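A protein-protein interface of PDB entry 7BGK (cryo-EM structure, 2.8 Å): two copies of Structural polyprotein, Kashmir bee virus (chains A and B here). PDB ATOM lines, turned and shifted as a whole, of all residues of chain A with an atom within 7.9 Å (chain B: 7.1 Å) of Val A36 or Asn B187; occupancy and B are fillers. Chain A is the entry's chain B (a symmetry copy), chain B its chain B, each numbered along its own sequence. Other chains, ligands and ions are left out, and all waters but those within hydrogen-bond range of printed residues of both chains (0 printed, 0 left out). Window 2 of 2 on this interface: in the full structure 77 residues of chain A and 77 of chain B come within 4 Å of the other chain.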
ATOM      1  N   SER A  18      30.846 -23.774 -25.987  1.00  0.00           N
ATOM      2  CA  SER A  18      32.103 -23.087 -25.749  1.00  0.00           C
ATOM      3  C   SER A  18      32.072 -22.468 -24.365  1.00  0.00           C
ATOM      4  O   SER A  18      31.013 -22.328 -23.750  1.00  0.00           O
ATOM      5  CB  SER A  18      32.341 -22.004 -26.803  1.00  0.00           C
ATOM      6  OG  SER A  18      32.478 -22.557 -28.097  1.00  0.00           O
ATOM      7  N   SER A  20      32.990 -19.119 -21.836  1.00  0.00           N
ATOM      8  CA  SER A  20      32.682 -17.706 -21.950  1.00  0.00           C
ATOM      9  C   SER A  20      33.041 -17.031 -20.633  1.00  0.00           C
ATOM     10  O   SER A  20      33.568 -17.660 -19.714  1.00  0.00           O
ATOM     11  CB  SER A  20      31.218 -17.500 -22.322  1.00  0.00           C
ATOM     12  OG  SER A  20      30.984 -17.841 -23.675  1.00  0.00           O
ATOM     13  N   ALA A  21      32.758 -15.735 -20.556  1.00  0.00           N
ATOM     14  CA  ALA A  21      33.065 -14.977 -19.356  1.00  0.00           C
ATOM     15  C   ALA A  21      32.303 -15.546 -18.169  1.00  0.00           C
ATOM     16  O   ALA A  21      31.111 -15.842 -18.260  1.00  0.00           O
ATOM     17  CB  ALA A  21      32.715 -13.509 -19.566  1.00  0.00           C
ATOM     18  N   GLU A  22      32.996 -15.668 -17.040  1.00  0.00           N
ATOM     19  CA  GLU A  22      32.570 -16.498 -15.924  1.00  0.00           C
ATOM     20  C   GLU A  22      31.575 -15.815 -14.995  1.00  0.00           C
ATOM     21  O   GLU A  22      31.298 -16.354 -13.921  1.00  0.00           O
ATOM     22  CB  GLU A  22      33.799 -16.941 -15.127  1.00  0.00           C
ATOM     23  CG  GLU A  22      34.523 -18.124 -15.733  1.00  0.00           C
ATOM     24  CD  GLU A  22      35.548 -18.735 -14.796  1.00  0.00           C
ATOM     25  OE1 GLU A  22      36.056 -19.834 -15.104  1.00  0.00           O
ATOM     26  OE2 GLU A  22      35.848 -18.117 -13.755  1.00  0.00           O
ATOM     27  N   ASN A  23      31.024 -14.663 -15.373  1.00  0.00           N
ATOM     28  CA  ASN A  23      30.024 -13.994 -14.540  1.00  0.00           C
ATOM     29  C   ASN A  23      29.168 -13.118 -15.452  1.00  0.00           C
ATOM     30  O   ASN A  23      29.582 -12.017 -15.819  1.00  0.00           O
ATOM     31  CB  ASN A  23      30.686 -13.181 -13.439  1.00  0.00           C
ATOM     32  CG  ASN A  23      29.713 -12.305 -12.690  1.00  0.00           C
ATOM     33  OD1 ASN A  23      29.895 -11.094 -12.594  1.00  0.00           O
ATOM     34  ND2 ASN A  23      28.676 -12.910 -12.152  1.00  0.00           N
ATOM     35  N   ALA A  24      27.987 -13.615 -15.802  1.00  0.00           N
ATOM     36  CA  ALA A  24      27.109 -12.959 -16.756  1.00  0.00           C
ATOM     37  C   ALA A  24      25.801 -12.562 -16.093  1.00  0.00           C
ATOM     38  O   ALA A  24      25.226 -13.332 -15.321  1.00  0.00           O
ATOM     39  CB  ALA A  24      26.816 -13.868 -17.939  1.00  0.00           C
ATOM     40  N   ILE A  25      25.340 -11.351 -16.397  1.00  0.00           N
ATOM     41  CA  ILE A  25      24.063 -10.868 -15.896  1.00  0.00           C
ATOM     42  C   ILE A  25      23.318 -10.166 -17.022  1.00  0.00           C
ATOM     43  O   ILE A  25      23.642  -9.029 -17.379  1.00  0.00           O
ATOM     44  CB  ILE A  25      24.250  -9.927 -14.697  1.00  0.00           C
ATOM     45  CG1 ILE A  25      24.892 -10.657 -13.527  1.00  0.00           C
ATOM     46  CG2 ILE A  25      22.927  -9.370 -14.244  1.00  0.00           C
ATOM     47  CD1 ILE A  25      25.587  -9.752 -12.595  1.00  0.00           C
ATOM     48  N   GLU A  26      22.325 -10.839 -17.590  1.00  0.00           N
ATOM     49  CA  GLU A  26      21.475 -10.267 -18.623  1.00  0.00           C
ATOM     50  C   GLU A  26      20.179  -9.782 -17.999  1.00  0.00           C
ATOM     51  O   GLU A  26      19.494 -10.541 -17.308  1.00  0.00           O
ATOM     52  CB  GLU A  26      21.187 -11.268 -19.741  1.00  0.00           C
ATOM     53  CG  GLU A  26      22.427 -11.831 -20.420  1.00  0.00           C
ATOM     54  CD  GLU A  26      23.086 -12.962 -19.647  1.00  0.00           C
ATOM     55  OE1 GLU A  26      22.485 -13.457 -18.669  1.00  0.00           O
ATOM     56  OE2 GLU A  26      24.213 -13.354 -20.015  1.00  0.00           O
ATOM     57  N   PHE A  33      18.555 -12.315 -15.423  1.00  0.00           N
ATOM     58  CA  PHE A  33      19.191 -13.618 -15.396  1.00  0.00           C
ATOM     59  C   PHE A  33      20.648 -13.479 -14.990  1.00  0.00           C
ATOM     60  O   PHE A  33      21.401 -12.720 -15.605  1.00  0.00           O
ATOM     61  CB  PHE A  33      19.117 -14.283 -16.764  1.00  0.00           C
ATOM     62  CG  PHE A  33      17.733 -14.523 -17.249  1.00  0.00           C
ATOM     63  CD1 PHE A  33      17.020 -15.618 -16.819  1.00  0.00           C
ATOM     64  CD2 PHE A  33      17.149 -13.668 -18.160  1.00  0.00           C
ATOM     65  CE1 PHE A  33      15.761 -15.845 -17.271  1.00  0.00           C
ATOM     66  CE2 PHE A  33      15.884 -13.897 -18.612  1.00  0.00           C
ATOM     67  CZ  PHE A  33      15.190 -14.985 -18.168  1.00  0.00           C
ATOM     68  N   HIS A  34      21.044 -14.221 -13.966  1.00  0.00           N
ATOM     69  CA  HIS A  34      22.446 -14.472 -13.687  1.00  0.00           C
ATOM     70  C   HIS A  34      22.798 -15.866 -14.179  1.00  0.00           C
ATOM     71  O   HIS A  34      22.085 -16.832 -13.892  1.00  0.00           O
ATOM     72  CB  HIS A  34      22.752 -14.343 -12.200  1.00  0.00           C
ATOM     73  CG  HIS A  34      24.169 -14.662 -11.849  1.00  0.00           C
ATOM     74  ND1 HIS A  34      24.528 -15.819 -11.196  1.00  0.00           N
ATOM     75  CD2 HIS A  34      25.317 -13.980 -12.067  1.00  0.00           C
ATOM     76  CE1 HIS A  34      25.837 -15.836 -11.026  1.00  0.00           C
ATOM     77  NE2 HIS A  34      26.340 -14.733 -11.546  1.00  0.00           N
ATOM     78  N   ASP A  35      23.885 -15.959 -14.932  1.00  0.00           N
ATOM     79  CA  ASP A  35      24.373 -17.215 -15.465  1.00  0.00           C
ATOM     80  C   ASP A  35      25.836 -17.379 -15.088  1.00  0.00           C
ATOM     81  O   ASP A  35      26.564 -16.398 -14.927  1.00  0.00           O
ATOM     82  CB  ASP A  35      24.204 -17.270 -16.979  1.00  0.00           C
ATOM     83  CG  ASP A  35      22.753 -17.202 -17.405  1.00  0.00           C
ATOM     84  OD1 ASP A  35      21.922 -17.914 -16.807  1.00  0.00           O
ATOM     85  OD2 ASP A  35      22.440 -16.430 -18.334  1.00  0.00           O
ATOM     86  N   VAL A  36      26.259 -18.633 -14.935  1.00  0.00           N
ATOM     87  CA  VAL A  36      27.638 -18.896 -14.539  1.00  0.00           C
ATOM     88  C   VAL A  36      28.596 -18.414 -15.617  1.00  0.00           C
ATOM     89  O   VAL A  36      29.663 -17.866 -15.320  1.00  0.00           O
ATOM     90  CB  VAL A  36      27.831 -20.392 -14.230  1.00  0.00           C
ATOM     91  CG1 VAL A  36      27.578 -21.240 -15.446  1.00  0.00           C
ATOM     92  CG2 VAL A  36      29.207 -20.643 -13.711  1.00  0.00           C
ATOM     93  N   GLU A  37      28.237 -18.617 -16.877  1.00  0.00           N
ATOM     94  CA  GLU A  37      28.987 -18.096 -18.001  1.00  0.00           C
ATOM     95  C   GLU A  37      28.020 -17.478 -18.997  1.00  0.00           C
ATOM     96  O   GLU A  37      26.813 -17.724 -18.958  1.00  0.00           O
ATOM     97  CB  GLU A  37      29.829 -19.181 -18.678  1.00  0.00           C
ATOM     98  CG  GLU A  37      31.068 -19.580 -17.913  1.00  0.00           C
ATOM     99  CD  GLU A  37      31.775 -20.760 -18.530  1.00  0.00           C
ATOM    100  OE1 GLU A  37      31.117 -21.792 -18.767  1.00  0.00           O
ATOM    101  OE2 GLU A  37      32.994 -20.657 -18.775  1.00  0.00           O
ATOM    102  N   THR A  38      28.567 -16.664 -19.883  1.00  0.00           N
ATOM    103  CA  THR A  38      27.745 -15.976 -20.862  1.00  0.00           C
ATOM    104  C   THR A  38      27.039 -16.996 -21.749  1.00  0.00           C
ATOM    105  O   THR A  38      27.700 -17.871 -22.323  1.00  0.00           O
ATOM    106  CB  THR A  38      28.599 -15.041 -21.713  1.00  0.00           C
ATOM    107  OG1 THR A  38      29.421 -14.234 -20.865  1.00  0.00           O
ATOM    108  CG2 THR A  38      27.737 -14.142 -22.552  1.00  0.00           C
ATOM    109  N   PRO A  39      25.716 -16.932 -21.876  1.00  0.00           N
ATOM    110  CA  PRO A  39      25.013 -17.894 -22.725  1.00  0.00           C
ATOM    111  C   PRO A  39      25.606 -17.947 -24.123  1.00  0.00           C
ATOM    112  O   PRO A  39      26.217 -16.990 -24.599  1.00  0.00           O
ATOM    113  CB  PRO A  39      23.580 -17.359 -22.746  1.00  0.00           C
ATOM    114  CG  PRO A  39      23.444 -16.624 -21.512  1.00  0.00           C
ATOM    115  CD  PRO A  39      24.771 -16.023 -21.211  1.00  0.00           C
ATOM    116  N   ASN A  40      25.420 -19.084 -24.779  1.00  0.00           N
ATOM    117  CA  ASN A  40      25.898 -19.279 -26.140  1.00  0.00           C
ATOM    118  C   ASN A  40      24.717 -19.046 -27.073  1.00  0.00           C
ATOM    119  O   ASN A  40      23.913 -19.937 -27.335  1.00  0.00           O
ATOM    120  CB  ASN A  40      26.506 -20.662 -26.317  1.00  0.00           C
ATOM    121  CG  ASN A  40      27.786 -20.829 -25.547  1.00  0.00           C
ATOM    122  OD1 ASN A  40      27.931 -20.330 -24.432  1.00  0.00           O
ATOM    123  ND2 ASN A  40      28.746 -21.498 -26.156  1.00  0.00           N
ATOM    124  N   ILE B 136      17.244 -20.941 -22.387  1.00  0.00           N
ATOM    125  CA  ILE B 136      17.161 -22.164 -21.600  1.00  0.00           C
ATOM    126  C   ILE B 136      18.242 -22.119 -20.530  1.00  0.00           C
ATOM    127  O   ILE B 136      19.421 -21.922 -20.846  1.00  0.00           O
ATOM    128  CB  ILE B 136      17.320 -23.408 -22.488  1.00  0.00           C
ATOM    129  CG1 ILE B 136      16.208 -23.455 -23.527  1.00  0.00           C
ATOM    130  CG2 ILE B 136      17.300 -24.660 -21.656  1.00  0.00           C
ATOM    131  CD1 ILE B 136      16.376 -24.515 -24.545  1.00  0.00           C
ATOM    132  N   VAL B 137      17.846 -22.295 -19.272  1.00  0.00           N
ATOM    133  CA  VAL B 137      18.779 -22.414 -18.158  1.00  0.00           C
ATOM    134  C   VAL B 137      18.752 -23.864 -17.705  1.00  0.00           C
ATOM    135  O   VAL B 137      17.761 -24.329 -17.131  1.00  0.00           O
ATOM    136  CB  VAL B 137      18.437 -21.471 -16.997  1.00  0.00           C
ATOM    137  CG1 VAL B 137      19.607 -21.423 -15.943  1.00  0.00           C
ATOM    138  CG2 VAL B 137      18.103 -20.104 -17.519  1.00  0.00           C
ATOM    139  N   LEU B 138      19.834 -24.579 -17.974  1.00  0.00           N
ATOM    140  CA  LEU B 138      20.012 -25.952 -17.542  1.00  0.00           C
ATOM    141  C   LEU B 138      20.914 -26.002 -16.319  1.00  0.00           C
ATOM    142  O   LEU B 138      21.779 -25.147 -16.127  1.00  0.00           O
ATOM    143  CB  LEU B 138      20.600 -26.797 -18.668  1.00  0.00           C
ATOM    144  CG  LEU B 138      20.917 -28.247 -18.329  1.00  0.00           C
ATOM    145  CD1 LEU B 138      20.531 -29.134 -19.456  1.00  0.00           C
ATOM    146  CD2 LEU B 138      22.388 -28.393 -18.053  1.00  0.00           C
ATOM    147  N   ASN B 139      20.694 -27.012 -15.483  1.00  0.00           N
ATOM    148  CA  ASN B 139      21.500 -27.214 -14.290  1.00  0.00           C
ATOM    149  C   ASN B 139      21.734 -28.701 -14.097  1.00  0.00           C
ATOM    150  O   ASN B 139      20.783 -29.488 -14.073  1.00  0.00           O
ATOM    151  CB  ASN B 139      20.827 -26.613 -13.056  1.00  0.00           C
ATOM    152  CG  ASN B 139      21.055 -25.126 -12.943  1.00  0.00           C
ATOM    153  OD1 ASN B 139      20.201 -24.326 -13.317  1.00  0.00           O
ATOM    154  ND2 ASN B 139      22.211 -24.745 -12.430  1.00  0.00           N
ATOM    155  N   ALA B 140      23.003 -29.075 -13.965  1.00  0.00           N
ATOM    156  CA  ALA B 140      23.404 -30.463 -13.810  1.00  0.00           C
ATOM    157  C   ALA B 140      24.685 -30.500 -12.997  1.00  0.00           C
ATOM    158  O   ALA B 140      25.653 -29.816 -13.340  1.00  0.00           O
ATOM    159  CB  ALA B 140      23.618 -31.127 -15.166  1.00  0.00           C
ATOM    160  N   LEU B 181      24.214 -27.510 -26.751  1.00  0.00           N
ATOM    161  CA  LEU B 181      23.927 -27.246 -25.342  1.00  0.00           C
ATOM    162  C   LEU B 181      24.508 -28.369 -24.488  1.00  0.00           C
ATOM    163  O   LEU B 181      23.835 -29.362 -24.206  1.00  0.00           O
ATOM    164  CB  LEU B 181      22.426 -27.093 -25.141  1.00  0.00           C
ATOM    165  CG  LEU B 181      21.850 -27.196 -23.732  1.00  0.00           C
ATOM    166  CD1 LEU B 181      22.444 -26.189 -22.798  1.00  0.00           C
ATOM    167  CD2 LEU B 181      20.356 -27.013 -23.809  1.00  0.00           C
ATOM    168  N   ASP B 182      25.758 -28.203 -24.073  1.00  0.00           N
ATOM    169  CA  ASP B 182      26.423 -29.157 -23.203  1.00  0.00           C
ATOM    170  C   ASP B 182      26.158 -28.812 -21.745  1.00  0.00           C
ATOM    171  O   ASP B 182      25.999 -27.646 -21.379  1.00  0.00           O
ATOM    172  CB  ASP B 182      27.924 -29.171 -23.472  1.00  0.00           C
ATOM    173  CG  ASP B 182      28.570 -30.500 -23.137  1.00  0.00           C
ATOM    174  OD1 ASP B 182      28.157 -31.136 -22.147  1.00  0.00           O
ATOM    175  OD2 ASP B 182      29.497 -30.910 -23.865  1.00  0.00           O
ATOM    176  N   PHE B 183      26.121 -29.848 -20.909  1.00  0.00           N
ATOM    177  CA  PHE B 183      25.750 -29.655 -19.514  1.00  0.00           C
ATOM    178  C   PHE B 183      26.862 -28.969 -18.732  1.00  0.00           C
ATOM    179  O   PHE B 183      26.592 -28.140 -17.857  1.00  0.00           O
ATOM    180  CB  PHE B 183      25.394 -30.999 -18.883  1.00  0.00           C
ATOM    181  CG  PHE B 183      24.199 -31.671 -19.499  1.00  0.00           C
ATOM    182  CD1 PHE B 183      23.477 -31.070 -20.510  1.00  0.00           C
ATOM    183  CD2 PHE B 183      23.799 -32.913 -19.062  1.00  0.00           C
ATOM    184  CE1 PHE B 183      22.394 -31.695 -21.063  1.00  0.00           C
ATOM    185  CE2 PHE B 183      22.717 -33.536 -19.620  1.00  0.00           C
ATOM    186  CZ  PHE B 183      22.016 -32.927 -20.616  1.00  0.00           C
ATOM    187  N   GLN B 184      28.116 -29.298 -19.032  1.00  0.00           N
ATOM    188  CA  GLN B 184      29.252 -28.785 -18.282  1.00  0.00           C
ATOM    189  C   GLN B 184      29.984 -27.652 -18.984  1.00  0.00           C
ATOM    190  O   GLN B 184      30.903 -27.075 -18.395  1.00  0.00           O
ATOM    191  CB  GLN B 184      30.242 -29.916 -17.987  1.00  0.00           C
ATOM    192  CG  GLN B 184      29.697 -31.036 -17.119  1.00  0.00           C
ATOM    193  CD  GLN B 184      28.866 -30.548 -15.960  1.00  0.00           C
ATOM    194  OE1 GLN B 184      29.199 -29.561 -15.308  1.00  0.00           O
ATOM    195  NE2 GLN B 184      27.776 -31.241 -15.693  1.00  0.00           N
ATOM    196  N   LEU B 185      29.616 -27.327 -20.219  1.00  0.00           N
ATOM    197  CA  LEU B 185      30.143 -26.163 -20.915  1.00  0.00           C
ATOM    198  C   LEU B 185      29.114 -25.045 -21.003  1.00  0.00           C
ATOM    199  O   LEU B 185      29.380 -23.920 -20.574  1.00  0.00           O
ATOM    200  CB  LEU B 185      30.614 -26.549 -22.322  1.00  0.00           C
ATOM    201  CG  LEU B 185      31.753 -27.551 -22.443  1.00  0.00           C
ATOM    202  CD1 LEU B 185      31.999 -27.856 -23.888  1.00  0.00           C
ATOM    203  CD2 LEU B 185      32.997 -27.016 -21.806  1.00  0.00           C
ATOM    204  N   ASP B 186      27.938 -25.334 -21.545  1.00  0.00           N
ATOM    205  CA  ASP B 186      26.892 -24.348 -21.785  1.00  0.00           C
ATOM    206  C   ASP B 186      25.743 -24.636 -20.825  1.00  0.00           C
ATOM    207  O   ASP B 186      24.788 -25.334 -21.162  1.00  0.00           O
ATOM    208  CB  ASP B 186      26.431 -24.388 -23.232  1.00  0.00           C
ATOM    209  CG  ASP B 186      27.574 -24.324 -24.208  1.00  0.00           C
ATOM    210  OD1 ASP B 186      28.468 -23.476 -24.017  1.00  0.00           O
ATOM    211  OD2 ASP B 186      27.583 -25.120 -25.168  1.00  0.00           O
ATOM    212  N   ASN B 187      25.847 -24.088 -19.619  1.00  0.00           N
ATOM    213  CA  ASN B 187      24.764 -24.161 -18.650  1.00  0.00           C
ATOM    214  C   ASN B 187      23.533 -23.393 -19.106  1.00  0.00           C
ATOM    215  O   ASN B 187      22.463 -23.560 -18.515  1.00  0.00           O
ATOM    216  CB  ASN B 187      25.249 -23.616 -17.310  1.00  0.00           C
ATOM    217  CG  ASN B 187      24.632 -24.320 -16.134  1.00  0.00           C
ATOM    218  OD1 ASN B 187      24.385 -25.524 -16.166  1.00  0.00           O
ATOM    219  ND2 ASN B 187      24.416 -23.576 -15.064  1.00  0.00           N
ATOM    220  N   SER B 188      23.660 -22.565 -20.137  1.00  0.00           N
ATOM    221  CA  SER B 188      22.572 -21.727 -20.607  1.00  0.00           C
ATOM    222  C   SER B 188      22.832 -21.358 -22.057  1.00  0.00           C
ATOM    223  O   SER B 188      23.966 -21.051 -22.430  1.00  0.00           O
ATOM    224  CB  SER B 188      22.432 -20.461 -19.764  1.00  0.00           C
ATOM    225  OG  SER B 188      21.461 -19.597 -20.316  1.00  0.00           O
ATOM    226  N   VAL B 189      21.779 -21.393 -22.864  1.00  0.00           N
ATOM    227  CA  VAL B 189      21.853 -21.011 -24.265  1.00  0.00           C
ATOM    228  C   VAL B 189      20.725 -20.048 -24.586  1.00  0.00           C
ATOM    229  O   VAL B 189      19.655 -20.079 -23.971  1.00  0.00           O
ATOM    230  CB  VAL B 189      21.798 -22.225 -25.211  1.00  0.00           C
ATOM    231  CG1 VAL B 189      22.980 -23.122 -24.983  1.00  0.00           C
ATOM    232  CG2 VAL B 189      20.510 -22.979 -25.038  1.00  0.00           C
ATOM    233  N   LEU B 236      15.631 -28.626 -16.567  1.00  0.00           N
ATOM    234  CA  LEU B 236      15.617 -27.559 -17.549  1.00  0.00           C
ATOM    235  C   LEU B 236      14.491 -26.585 -17.238  1.00  0.00           C
ATOM    236  O   LEU B 236      13.497 -26.931 -16.598  1.00  0.00           O
ATOM    237  CB  LEU B 236      15.435 -28.119 -18.957  1.00  0.00           C
ATOM    238  CG  LEU B 236      16.679 -28.648 -19.646  1.00  0.00           C
ATOM    239  CD1 LEU B 236      16.312 -29.776 -20.549  1.00  0.00           C
ATOM    240  CD2 LEU B 236      17.304 -27.551 -20.441  1.00  0.00           C
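N of Ser A18 lies within hydrogen-bond range of OD1 of Asp B186.
OD1 of Asp B186 sits at hydrogen-bond distance from ND2 of Asn A40 (2.9 Å).
The backbone carbonyl oxygen (O) of Ser B188 sits at hydrogen-bond distance from the backbone NH (N) of Asn A40 (3.4 Å).
The side-chain carboxylate (OE1) of Glu A37 sits close to the backbone carbonyl oxygen (O) of Leu B185, at 3.3 Å.
The backbone carbonyl oxygen (O) of Ile B136 lies within hydrogen-bond range of the side-chain hydroxyl (OG) of Ser B188 (3.1 Å).
N of Ile B136 lies within hydrogen-bond range of O of Val B189 (3.0 Å).
The backbone NH of Ser A18 sits close to the side-chain amide nitrogen of Asn A40.
The backbone carbonyl oxygen (O) of Glu A22 sits close to the backbone carbonyl oxygen (O) of Val A36.
The backbone carbonyl oxygen (O) of Val A36 is in hydrogen-bond range of the backbone NH (N) of Asn A23, at 3.5 Å.
O of Thr A38 sits close to OD1 of Asn A40.
O of Ser A18 touches O of Leu B185, at 3.9 Å.
OD2 of Asp A35 touches OG of Ser B188, 3.9 Å away.
Val A36 touches Asn B187 (CG1 to CB, 3.8 Å).
CA of Pro A39 touches O of Ser B188 (3.3 Å).
Asn A40 touches Val B189.
Of the printed residues of chain B, Asn A40 touches Asp B186, Ser B188 and Val B189.
Of the printed residues of chain B, Ser A18 touches Leu B185 (3.9 Å) and Asp B186 (2.8 Å).
Of the printed residues of chain A, Val B189 touches Asn A40.
Leu B236 touches none of the printed residues of chain A.
His A34 touches none of the printed residues of chain B.
The nearest residue of chain B that does not touch Val A36 is Leu B185 (6.1 Å).
The nearest printed residue of chain B that does not touch Pro A39 is Val B189 (4.3 Å).
Of the 15 printed residues of chain B, 5 touch a printed residue of chain A.
No position is printed for both chains.
Of the 9 pairs that touch across the chains among the printed residues, none has its exchanged pair printed and touching as well.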
